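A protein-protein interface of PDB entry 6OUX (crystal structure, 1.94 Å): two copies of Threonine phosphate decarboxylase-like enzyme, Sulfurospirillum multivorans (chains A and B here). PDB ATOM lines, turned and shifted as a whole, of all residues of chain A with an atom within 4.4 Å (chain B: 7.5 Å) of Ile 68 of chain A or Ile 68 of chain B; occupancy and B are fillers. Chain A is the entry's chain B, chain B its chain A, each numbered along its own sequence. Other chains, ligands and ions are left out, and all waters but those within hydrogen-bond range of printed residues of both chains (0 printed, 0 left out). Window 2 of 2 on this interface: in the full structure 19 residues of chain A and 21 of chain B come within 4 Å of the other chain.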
ATOM      1  N   ILE A  63     -31.121 -35.416 -26.952  1.00  0.00           N
ATOM      2  CA  ILE A  63     -30.463 -34.179 -26.562  1.00  0.00           C
ATOM      3  C   ILE A  63     -29.123 -34.420 -25.925  1.00  0.00           C
ATOM      4  O   ILE A  63     -28.187 -33.712 -26.223  1.00  0.00           O
ATOM      5  CB  ILE A  63     -31.340 -33.284 -25.658  1.00  0.00           C
ATOM      6  CG1 ILE A  63     -32.462 -32.703 -26.522  1.00  0.00           C
ATOM      7  CG2 ILE A  63     -30.512 -32.160 -25.065  1.00  0.00           C
ATOM      8  CD1 ILE A  63     -33.482 -31.843 -25.863  1.00  0.00           C
ATOM      9  N   ASP A  64     -29.059 -35.385 -25.025  1.00  0.00           N
ATOM     10  CA  ASP A  64     -27.820 -35.777 -24.378  1.00  0.00           C
ATOM     11  C   ASP A  64     -26.742 -36.301 -25.375  1.00  0.00           C
ATOM     12  O   ASP A  64     -25.609 -35.838 -25.352  1.00  0.00           O
ATOM     13  CB  ASP A  64     -28.138 -36.816 -23.305  1.00  0.00           C
ATOM     14  CG  ASP A  64     -26.904 -37.376 -22.695  1.00  0.00           C
ATOM     15  OD1 ASP A  64     -26.052 -36.606 -22.318  1.00  0.00           O
ATOM     16  OD2 ASP A  64     -26.764 -38.587 -22.646  1.00  0.00           O
ATOM     17  N   GLU A  66     -26.693 -35.805 -28.760  1.00  0.00           N
ATOM     18  CA  GLU A  66     -26.376 -34.876 -29.848  1.00  0.00           C
ATOM     19  C   GLU A  66     -25.912 -33.479 -29.425  1.00  0.00           C
ATOM     20  O   GLU A  66     -25.198 -32.837 -30.181  1.00  0.00           O
ATOM     21  CB  GLU A  66     -27.554 -34.787 -30.819  1.00  0.00           C
ATOM     22  CG  GLU A  66     -27.893 -36.132 -31.425  1.00  0.00           C
ATOM     23  CD  GLU A  66     -28.941 -36.071 -32.531  1.00  0.00           C
ATOM     24  OE1 GLU A  66     -29.670 -35.073 -32.627  1.00  0.00           O
ATOM     25  OE2 GLU A  66     -29.058 -37.039 -33.287  1.00  0.00           O
ATOM     26  N   LEU A  67     -26.318 -33.016 -28.243  1.00  0.00           N
ATOM     27  CA  LEU A  67     -25.976 -31.670 -27.730  1.00  0.00           C
ATOM     28  C   LEU A  67     -25.090 -31.601 -26.467  1.00  0.00           C
ATOM     29  O   LEU A  67     -24.193 -30.752 -26.388  1.00  0.00           O
ATOM     30  CB  LEU A  67     -27.256 -30.893 -27.441  1.00  0.00           C
ATOM     31  CG  LEU A  67     -28.207 -30.633 -28.607  1.00  0.00           C
ATOM     32  CD1 LEU A  67     -29.267 -29.635 -28.174  1.00  0.00           C
ATOM     33  CD2 LEU A  67     -27.446 -30.123 -29.832  1.00  0.00           C
ATOM     34  N   ILE A  68     -25.349 -32.456 -25.481  1.00  0.00           N
ATOM     35  CA  ILE A  68     -24.612 -32.430 -24.188  1.00  0.00           C
ATOM     36  C   ILE A  68     -23.252 -33.162 -24.299  1.00  0.00           C
ATOM     37  O   ILE A  68     -22.223 -32.617 -23.909  1.00  0.00           O
ATOM     38  CB  ILE A  68     -25.472 -32.958 -22.986  1.00  0.00           C
ATOM     39  CG1 ILE A  68     -26.500 -31.923 -22.497  1.00  0.00           C
ATOM     40  CG2 ILE A  68     -24.625 -33.257 -21.751  1.00  0.00           C
ATOM     41  CD1 ILE A  68     -27.411 -31.329 -23.542  1.00  0.00           C
ATOM     42  N   GLN A  69     -23.244 -34.368 -24.853  1.00  0.00           N
ATOM     43  CA  GLN A  69     -22.010 -35.153 -25.012  1.00  0.00           C
ATOM     44  C   GLN A  69     -21.063 -34.670 -26.137  1.00  0.00           C
ATOM     45  O   GLN A  69     -20.036 -35.303 -26.370  1.00  0.00           O
ATOM     46  CB  GLN A  69     -22.347 -36.635 -25.242  1.00  0.00           C
ATOM     47  CG  GLN A  69     -22.904 -37.357 -24.025  1.00  0.00           C
ATOM     48  CD  GLN A  69     -21.988 -37.255 -22.816  1.00  0.00           C
ATOM     49  OE1 GLN A  69     -22.249 -36.469 -21.909  1.00  0.00           O
ATOM     50  NE2 GLN A  69     -20.888 -38.024 -22.810  1.00  0.00           N
ATOM     51  N   THR A  70     -21.434 -33.591 -26.844  1.00  0.00           N
ATOM     52  CA  THR A  70     -20.573 -32.909 -27.821  1.00  0.00           C
ATOM     53  C   THR A  70     -20.433 -31.406 -27.494  1.00  0.00           C
ATOM     54  O   THR A  70     -19.901 -30.639 -28.287  1.00  0.00           O
ATOM     55  CB  THR A  70     -21.021 -33.151 -29.304  1.00  0.00           C
ATOM     56  OG1 THR A  70     -22.412 -33.478 -29.381  1.00  0.00           O
ATOM     57  CG2 THR A  70     -20.272 -34.306 -29.937  1.00  0.00           C
ATOM     58  N   ASN A  71     -20.864 -30.990 -26.314  1.00  0.00           N
ATOM     59  CA  ASN A  71     -20.836 -29.554 -25.896  1.00  0.00           C
ATOM     60  C   ASN A  71     -21.556 -28.494 -26.781  1.00  0.00           C
ATOM     61  O   ASN A  71     -21.605 -27.323 -26.391  1.00  0.00           O
ATOM     62  CB  ASN A  71     -19.380 -29.094 -25.593  1.00  0.00           C
ATOM     63  CG  ASN A  71     -19.296 -28.097 -24.430  1.00  0.00           C
ATOM     64  OD1 ASN A  71     -19.627 -28.414 -23.297  1.00  0.00           O
ATOM     65  ND2 ASN A  71     -18.820 -26.889 -24.713  1.00  0.00           N
ATOM     66  N   TYR A  73     -24.245 -26.420 -27.191  1.00  0.00           N
ATOM     67  CA  TYR A  73     -25.421 -25.954 -26.522  1.00  0.00           C
ATOM     68  C   TYR A  73     -25.201 -24.514 -26.131  1.00  0.00           C
ATOM     69  O   TYR A  73     -26.110 -23.859 -25.619  1.00  0.00           O
ATOM     70  CB  TYR A  73     -25.785 -26.830 -25.296  1.00  0.00           C
ATOM     71  CG  TYR A  73     -24.821 -26.740 -24.131  1.00  0.00           C
ATOM     72  CD1 TYR A  73     -23.792 -27.667 -23.970  1.00  0.00           C
ATOM     73  CD2 TYR A  73     -24.929 -25.712 -23.205  1.00  0.00           C
ATOM     74  CE1 TYR A  73     -22.899 -27.551 -22.915  1.00  0.00           C
ATOM     75  CE2 TYR A  73     -24.059 -25.602 -22.137  1.00  0.00           C
ATOM     76  CZ  TYR A  73     -23.048 -26.515 -21.992  1.00  0.00           C
ATOM     77  OH  TYR A  73     -22.193 -26.380 -20.907  1.00  0.00           O
ATOM     78  N   LEU B  60     -22.433 -19.044 -18.934  1.00  0.00           N
ATOM     79  CA  LEU B  60     -22.236 -20.402 -19.504  1.00  0.00           C
ATOM     80  C   LEU B  60     -21.597 -21.356 -18.490  1.00  0.00           C
ATOM     81  O   LEU B  60     -21.918 -22.562 -18.436  1.00  0.00           O
ATOM     82  CB  LEU B  60     -21.403 -20.372 -20.766  1.00  0.00           C
ATOM     83  CG  LEU B  60     -22.135 -19.747 -21.978  1.00  0.00           C
ATOM     84  CD1 LEU B  60     -21.120 -19.427 -23.053  1.00  0.00           C
ATOM     85  CD2 LEU B  60     -23.237 -20.722 -22.448  1.00  0.00           C
ATOM     86  N   TYR B  62     -21.920 -21.195 -15.136  1.00  0.00           N
ATOM     87  CA  TYR B  62     -22.970 -21.608 -14.253  1.00  0.00           C
ATOM     88  C   TYR B  62     -23.902 -22.663 -14.876  1.00  0.00           C
ATOM     89  O   TYR B  62     -24.310 -23.639 -14.205  1.00  0.00           O
ATOM     90  CB  TYR B  62     -23.800 -20.427 -13.742  1.00  0.00           C
ATOM     91  CG  TYR B  62     -23.237 -19.686 -12.566  1.00  0.00           C
ATOM     92  CD1 TYR B  62     -22.371 -18.605 -12.706  1.00  0.00           C
ATOM     93  CD2 TYR B  62     -23.611 -20.027 -11.308  1.00  0.00           C
ATOM     94  CE1 TYR B  62     -21.901 -17.918 -11.621  1.00  0.00           C
ATOM     95  CE2 TYR B  62     -23.152 -19.348 -10.216  1.00  0.00           C
ATOM     96  CZ  TYR B  62     -22.294 -18.313 -10.381  1.00  0.00           C
ATOM     97  OH  TYR B  62     -21.899 -17.695  -9.272  1.00  0.00           O
ATOM     98  N   ILE B  63     -24.204 -22.496 -16.166  1.00  0.00           N
ATOM     99  CA  ILE B  63     -25.000 -23.476 -16.874  1.00  0.00           C
ATOM    100  C   ILE B  63     -24.274 -24.861 -16.902  1.00  0.00           C
ATOM    101  O   ILE B  63     -24.866 -25.873 -16.584  1.00  0.00           O
ATOM    102  CB  ILE B  63     -25.370 -22.977 -18.253  1.00  0.00           C
ATOM    103  CG1 ILE B  63     -26.307 -21.785 -18.115  1.00  0.00           C
ATOM    104  CG2 ILE B  63     -26.033 -24.089 -19.055  1.00  0.00           C
ATOM    105  CD1 ILE B  63     -26.657 -21.117 -19.435  1.00  0.00           C
ATOM    106  N   ASP B  64     -23.009 -24.857 -17.286  1.00  0.00           N
ATOM    107  CA  ASP B  64     -22.250 -26.057 -17.378  1.00  0.00           C
ATOM    108  C   ASP B  64     -22.234 -26.749 -16.045  1.00  0.00           C
ATOM    109  O   ASP B  64     -22.496 -27.955 -15.986  1.00  0.00           O
ATOM    110  CB  ASP B  64     -20.826 -25.744 -17.816  1.00  0.00           C
ATOM    111  CG  ASP B  64     -19.977 -26.981 -18.048  1.00  0.00           C
ATOM    112  OD1 ASP B  64     -20.520 -28.052 -18.283  1.00  0.00           O
ATOM    113  OD2 ASP B  64     -18.729 -26.871 -17.987  1.00  0.00           O
ATOM    114  N   ARG B  65     -21.914 -25.993 -14.992  1.00  0.00           N
ATOM    115  CA  ARG B  65     -21.712 -26.563 -13.666  1.00  0.00           C
ATOM    116  C   ARG B  65     -23.030 -26.980 -13.036  1.00  0.00           C
ATOM    117  O   ARG B  65     -23.102 -28.033 -12.411  1.00  0.00           O
ATOM    118  CB  ARG B  65     -20.897 -25.647 -12.721  1.00  0.00           C
ATOM    119  CG  ARG B  65     -19.400 -25.450 -13.111  1.00  0.00           C
ATOM    120  CD  ARG B  65     -18.686 -24.135 -12.575  1.00  0.00           C
ATOM    121  NE  ARG B  65     -19.387 -23.909 -11.377  1.00  0.00           N
ATOM    122  CZ  ARG B  65     -20.151 -22.921 -10.987  1.00  0.00           C
ATOM    123  NH1 ARG B  65     -20.768 -23.195  -9.900  1.00  0.00           N
ATOM    124  NH2 ARG B  65     -20.211 -21.700 -11.498  1.00  0.00           N
ATOM    125  N   GLU B  66     -24.053 -26.180 -13.202  1.00  0.00           N
ATOM    126  CA  GLU B  66     -25.315 -26.397 -12.495  1.00  0.00           C
ATOM    127  C   GLU B  66     -26.393 -27.166 -13.289  1.00  0.00           C
ATOM    128  O   GLU B  66     -27.313 -27.739 -12.684  1.00  0.00           O
ATOM    129  CB  GLU B  66     -25.930 -25.089 -11.992  1.00  0.00           C
ATOM    130  CG  GLU B  66     -25.045 -24.298 -11.036  1.00  0.00           C
ATOM    131  CD  GLU B  66     -25.749 -23.084 -10.422  1.00  0.00           C
ATOM    132  OE1 GLU B  66     -26.815 -22.696 -10.903  1.00  0.00           O
ATOM    133  OE2 GLU B  66     -25.206 -22.466  -9.474  1.00  0.00           O
ATOM    134  N   LEU B  67     -26.294 -27.153 -14.611  1.00  0.00           N
ATOM    135  CA  LEU B  67     -27.337 -27.812 -15.421  1.00  0.00           C
ATOM    136  C   LEU B  67     -26.840 -28.969 -16.200  1.00  0.00           C
ATOM    137  O   LEU B  67     -27.522 -29.986 -16.296  1.00  0.00           O
ATOM    138  CB  LEU B  67     -27.994 -26.821 -16.406  1.00  0.00           C
ATOM    139  CG  LEU B  67     -28.804 -25.699 -15.755  1.00  0.00           C
ATOM    140  CD1 LEU B  67     -29.476 -24.893 -16.842  1.00  0.00           C
ATOM    141  CD2 LEU B  67     -29.851 -26.130 -14.757  1.00  0.00           C
ATOM    142  N   ILE B  68     -25.666 -28.831 -16.788  1.00  0.00           N
ATOM    143  CA  ILE B  68     -25.205 -29.818 -17.716  1.00  0.00           C
ATOM    144  C   ILE B  68     -24.590 -30.974 -16.977  1.00  0.00           C
ATOM    145  O   ILE B  68     -25.041 -32.094 -17.161  1.00  0.00           O
ATOM    146  CB  ILE B  68     -24.221 -29.249 -18.718  1.00  0.00           C
ATOM    147  CG1 ILE B  68     -24.870 -28.114 -19.533  1.00  0.00           C
ATOM    148  CG2 ILE B  68     -23.700 -30.331 -19.614  1.00  0.00           C
ATOM    149  CD1 ILE B  68     -26.131 -28.439 -20.284  1.00  0.00           C
ATOM    150  N   GLN B  69     -23.583 -30.706 -16.146  1.00  0.00           N
ATOM    151  CA  GLN B  69     -22.865 -31.795 -15.437  1.00  0.00           C
ATOM    152  C   GLN B  69     -23.706 -32.492 -14.376  1.00  0.00           C
ATOM    153  O   GLN B  69     -23.417 -33.600 -13.991  1.00  0.00           O
ATOM    154  CB  GLN B  69     -21.613 -31.248 -14.754  1.00  0.00           C
ATOM    155  CG  GLN B  69     -20.567 -30.822 -15.707  1.00  0.00           C
ATOM    156  CD  GLN B  69     -19.260 -30.506 -15.010  1.00  0.00           C
ATOM    157  OE1 GLN B  69     -19.261 -29.866 -13.929  1.00  0.00           O
ATOM    158  NE2 GLN B  69     -18.129 -30.944 -15.627  1.00  0.00           N
ATOM    159  N   THR B  70     -24.737 -31.846 -13.879  1.00  0.00           N
ATOM    160  CA  THR B  70     -25.619 -32.469 -12.920  1.00  0.00           C
ATOM    161  C   THR B  70     -26.851 -33.150 -13.563  1.00  0.00           C
ATOM    162  O   THR B  70     -27.657 -33.691 -12.858  1.00  0.00           O
ATOM    163  CB  THR B  70     -26.212 -31.395 -12.062  1.00  0.00           C
ATOM    164  OG1 THR B  70     -27.019 -30.546 -12.930  1.00  0.00           O
ATOM    165  CG2 THR B  70     -25.106 -30.549 -11.422  1.00  0.00           C
ATOM    166  N   ASN B  71     -27.075 -32.990 -14.865  1.00  0.00           N
ATOM    167  CA  ASN B  71     -28.348 -33.426 -15.473  1.00  0.00           C
ATOM    168  C   ASN B  71     -29.633 -32.626 -15.046  1.00  0.00           C
ATOM    169  O   ASN B  71     -30.760 -33.014 -15.403  1.00  0.00           O
ATOM    170  CB  ASN B  71     -28.527 -34.978 -15.316  1.00  0.00           C
ATOM    171  CG  ASN B  71     -27.490 -35.790 -16.143  1.00  0.00           C
ATOM    172  OD1 ASN B  71     -27.016 -36.854 -15.724  1.00  0.00           O
ATOM    173  ND2 ASN B  71     -27.125 -35.282 -17.296  1.00  0.00           N
ATOM    174  N   ALA B  72     -29.482 -31.466 -14.396  1.00  0.00           N
ATOM    175  CA  ALA B  72     -30.649 -30.658 -14.039  1.00  0.00           C
ATOM    176  C   ALA B  72     -31.281 -30.020 -15.271  1.00  0.00           C
ATOM    177  O   ALA B  72     -32.424 -29.654 -15.225  1.00  0.00           O
ATOM    178  CB  ALA B  72     -30.305 -29.583 -12.992  1.00  0.00           C
ATOM    179  N   TYR B  73     -30.513 -29.879 -16.359  1.00  0.00           N
ATOM    180  CA  TYR B  73     -31.075 -29.455 -17.644  1.00  0.00           C
ATOM    181  C   TYR B  73     -32.322 -30.230 -18.073  1.00  0.00           C
ATOM    182  O   TYR B  73     -33.142 -29.653 -18.783  1.00  0.00           O
ATOM    183  CB  TYR B  73     -30.036 -29.425 -18.752  1.00  0.00           C
ATOM    184  CG  TYR B  73     -29.803 -30.743 -19.382  1.00  0.00           C
ATOM    185  CD1 TYR B  73     -28.904 -31.648 -18.810  1.00  0.00           C
ATOM    186  CD2 TYR B  73     -30.541 -31.152 -20.483  1.00  0.00           C
ATOM    187  CE1 TYR B  73     -28.710 -32.904 -19.362  1.00  0.00           C
ATOM    188  CE2 TYR B  73     -30.335 -32.394 -21.037  1.00  0.00           C
ATOM    189  CZ  TYR B  73     -29.419 -33.257 -20.489  1.00  0.00           C
ATOM    190  OH  TYR B  73     -29.239 -34.497 -21.006  1.00  0.00           O
ATOM    191  N   LYS B  74     -32.451 -31.503 -17.654  1.00  0.00           N
ATOM    192  CA  LYS B  74     -33.563 -32.378 -18.035  1.00  0.00           C
ATOM    193  C   LYS B  74     -34.912 -31.804 -17.578  1.00  0.00           C
ATOM    194  O   LYS B  74     -35.824 -31.676 -18.360  1.00  0.00           O
ATOM    195  CB  LYS B  74     -33.356 -33.783 -17.495  1.00  0.00           C
ATOM    196  CG  LYS B  74     -32.208 -34.474 -18.220  1.00  0.00           C
ATOM    197  CD  LYS B  74     -32.037 -35.937 -17.860  1.00  0.00           C
ATOM    198  CE  LYS B  74     -30.894 -36.523 -18.683  1.00  0.00           C
ATOM    199  NZ  LYS B  74     -30.615 -37.935 -18.274  1.00  0.00           N
ATOM    200  N   LEU B  77     -35.954 -28.473 -19.355  1.00  0.00           N
ATOM    201  CA  LEU B  77     -36.567 -28.640 -20.691  1.00  0.00           C
ATOM    202  C   LEU B  77     -37.943 -29.307 -20.659  1.00  0.00           C
ATOM    203  O   LEU B  77     -38.761 -29.078 -21.530  1.00  0.00           O
ATOM    204  CB  LEU B  77     -35.604 -29.408 -21.584  1.00  0.00           C
ATOM    205  CG  LEU B  77     -34.251 -28.670 -21.904  1.00  0.00           C
ATOM    206  CD1 LEU B  77     -33.325 -29.528 -22.763  1.00  0.00           C
ATOM    207  CD2 LEU B  77     -34.466 -27.306 -22.552  1.00  0.00           C
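The backbone carbonyl oxygen (O) of Leu 67 of chain B sits at hydrogen-bond distance from the backbone NH (N) of Tyr 73 of chain B, 3.0 Å away. The backbone NH of Gln 69 of chain A lies within hydrogen-bond range of the backbone carbonyl oxygen of Asp 64 of chain A (2.8 Å). The backbone carbonyl oxygen (O) of Ile 63 of chain B is in hydrogen-bond range of the backbone NH (N) of Ile 68 of chain B, at 3.1 Å. O of Asp 64 of chain B lies within hydrogen-bond range of N of Gln 69 of chain B (3.0 Å). The backbone carbonyl oxygen of Ile 63 of chain A lies within hydrogen-bond range of the backbone NH of Ile 68 of chain A (3.2 Å).
Among the printed residues, merely in contact across the chains: Tyr 73 of chain A with Asp 64 of chain B (3.4 Å), Asp 64 of chain A with Tyr 73 of chain B (3.4 Å), Tyr 73 of chain A with Ile 68 of chain B (3.5 Å), Ile 68 of chain A with Ile 68 of chain B (3.7 Å), Ile 68 of chain A with Tyr 73 of chain B (3.8 Å), Ile 63 of chain A with Leu 77 of chain B (3.9 Å) and Tyr 73 of chain A with Ile 63 of chain B (3.96 Å).
Printed residues of chain B within 4 Å of Ile 68 of chain A: Ile 68 and Tyr 73. Printed residues of chain A within 4 Å of Ile 68 of chain B: Ile 68 (3.7 Å) and Tyr 73 (3.5 Å). Of the printed residues of chain A, Tyr 73 of chain B touches Asp 64 and Ile 68. Printed residues of chain B within 4 Å of Asp 64 of chain A: Tyr 73. Of the printed residues of chain A, Leu 77 of chain B touches Ile 63. Of the printed residues of chain A, Asp 64 of chain B touches Tyr 73. Thr 70 of chain A touches none of the printed residues of chain B. The nearest residue of chain B that does not touch Ile 68 of chain A is Asn 71 of chain B (5.5 Å). The nearest printed residue of chain A that does not touch Ile 68 of chain B is Asn 71 of chain A (5.8 Å). The nearest printed residue of chain A that does not touch Ile 63 of chain B is Ile 68 of chain A (8.6 Å).
Printed residues of chain A that touch a printed residue of chain B: Ile 63, Asp 64, Ile 68 and Tyr 73. Hydrophobic or aromatic side chains of chain A that line the printed part of chain B: Ile 63, Ile 68 and Tyr 73. Printed residues of chain B that touch a printed residue of chain A: Ile 63, Asp 64, Ile 68, Tyr 73 and Leu 77. Hydrophobic or aromatic side chains of chain B that line the printed part of chain A: Ile 63, Ile 68, Tyr 73 and Leu 77.
Asp 64 of chain A touches Tyr 73 of chain B, and with the chains exchanged Tyr 73 of chain A touches Asp 64 of chain B. Ile 68 of chain A touches its own counterpart, Ile 68 of chain B. Ile 68 of chain A touches Tyr 73 of chain B, and with the chains exchanged Tyr 73 of chain A touches Ile 68 of chain B. Tyr 73 of chain A touches Ile 63 of chain B, but with the chains exchanged Ile 63 of chain A does not touch Tyr 73 of chain B (4.04 Å). 9 positions are printed for both chains. Of the 7 pairs that touch across the chains among the printed residues, 5 have their exchanged pair printed and touching as well.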
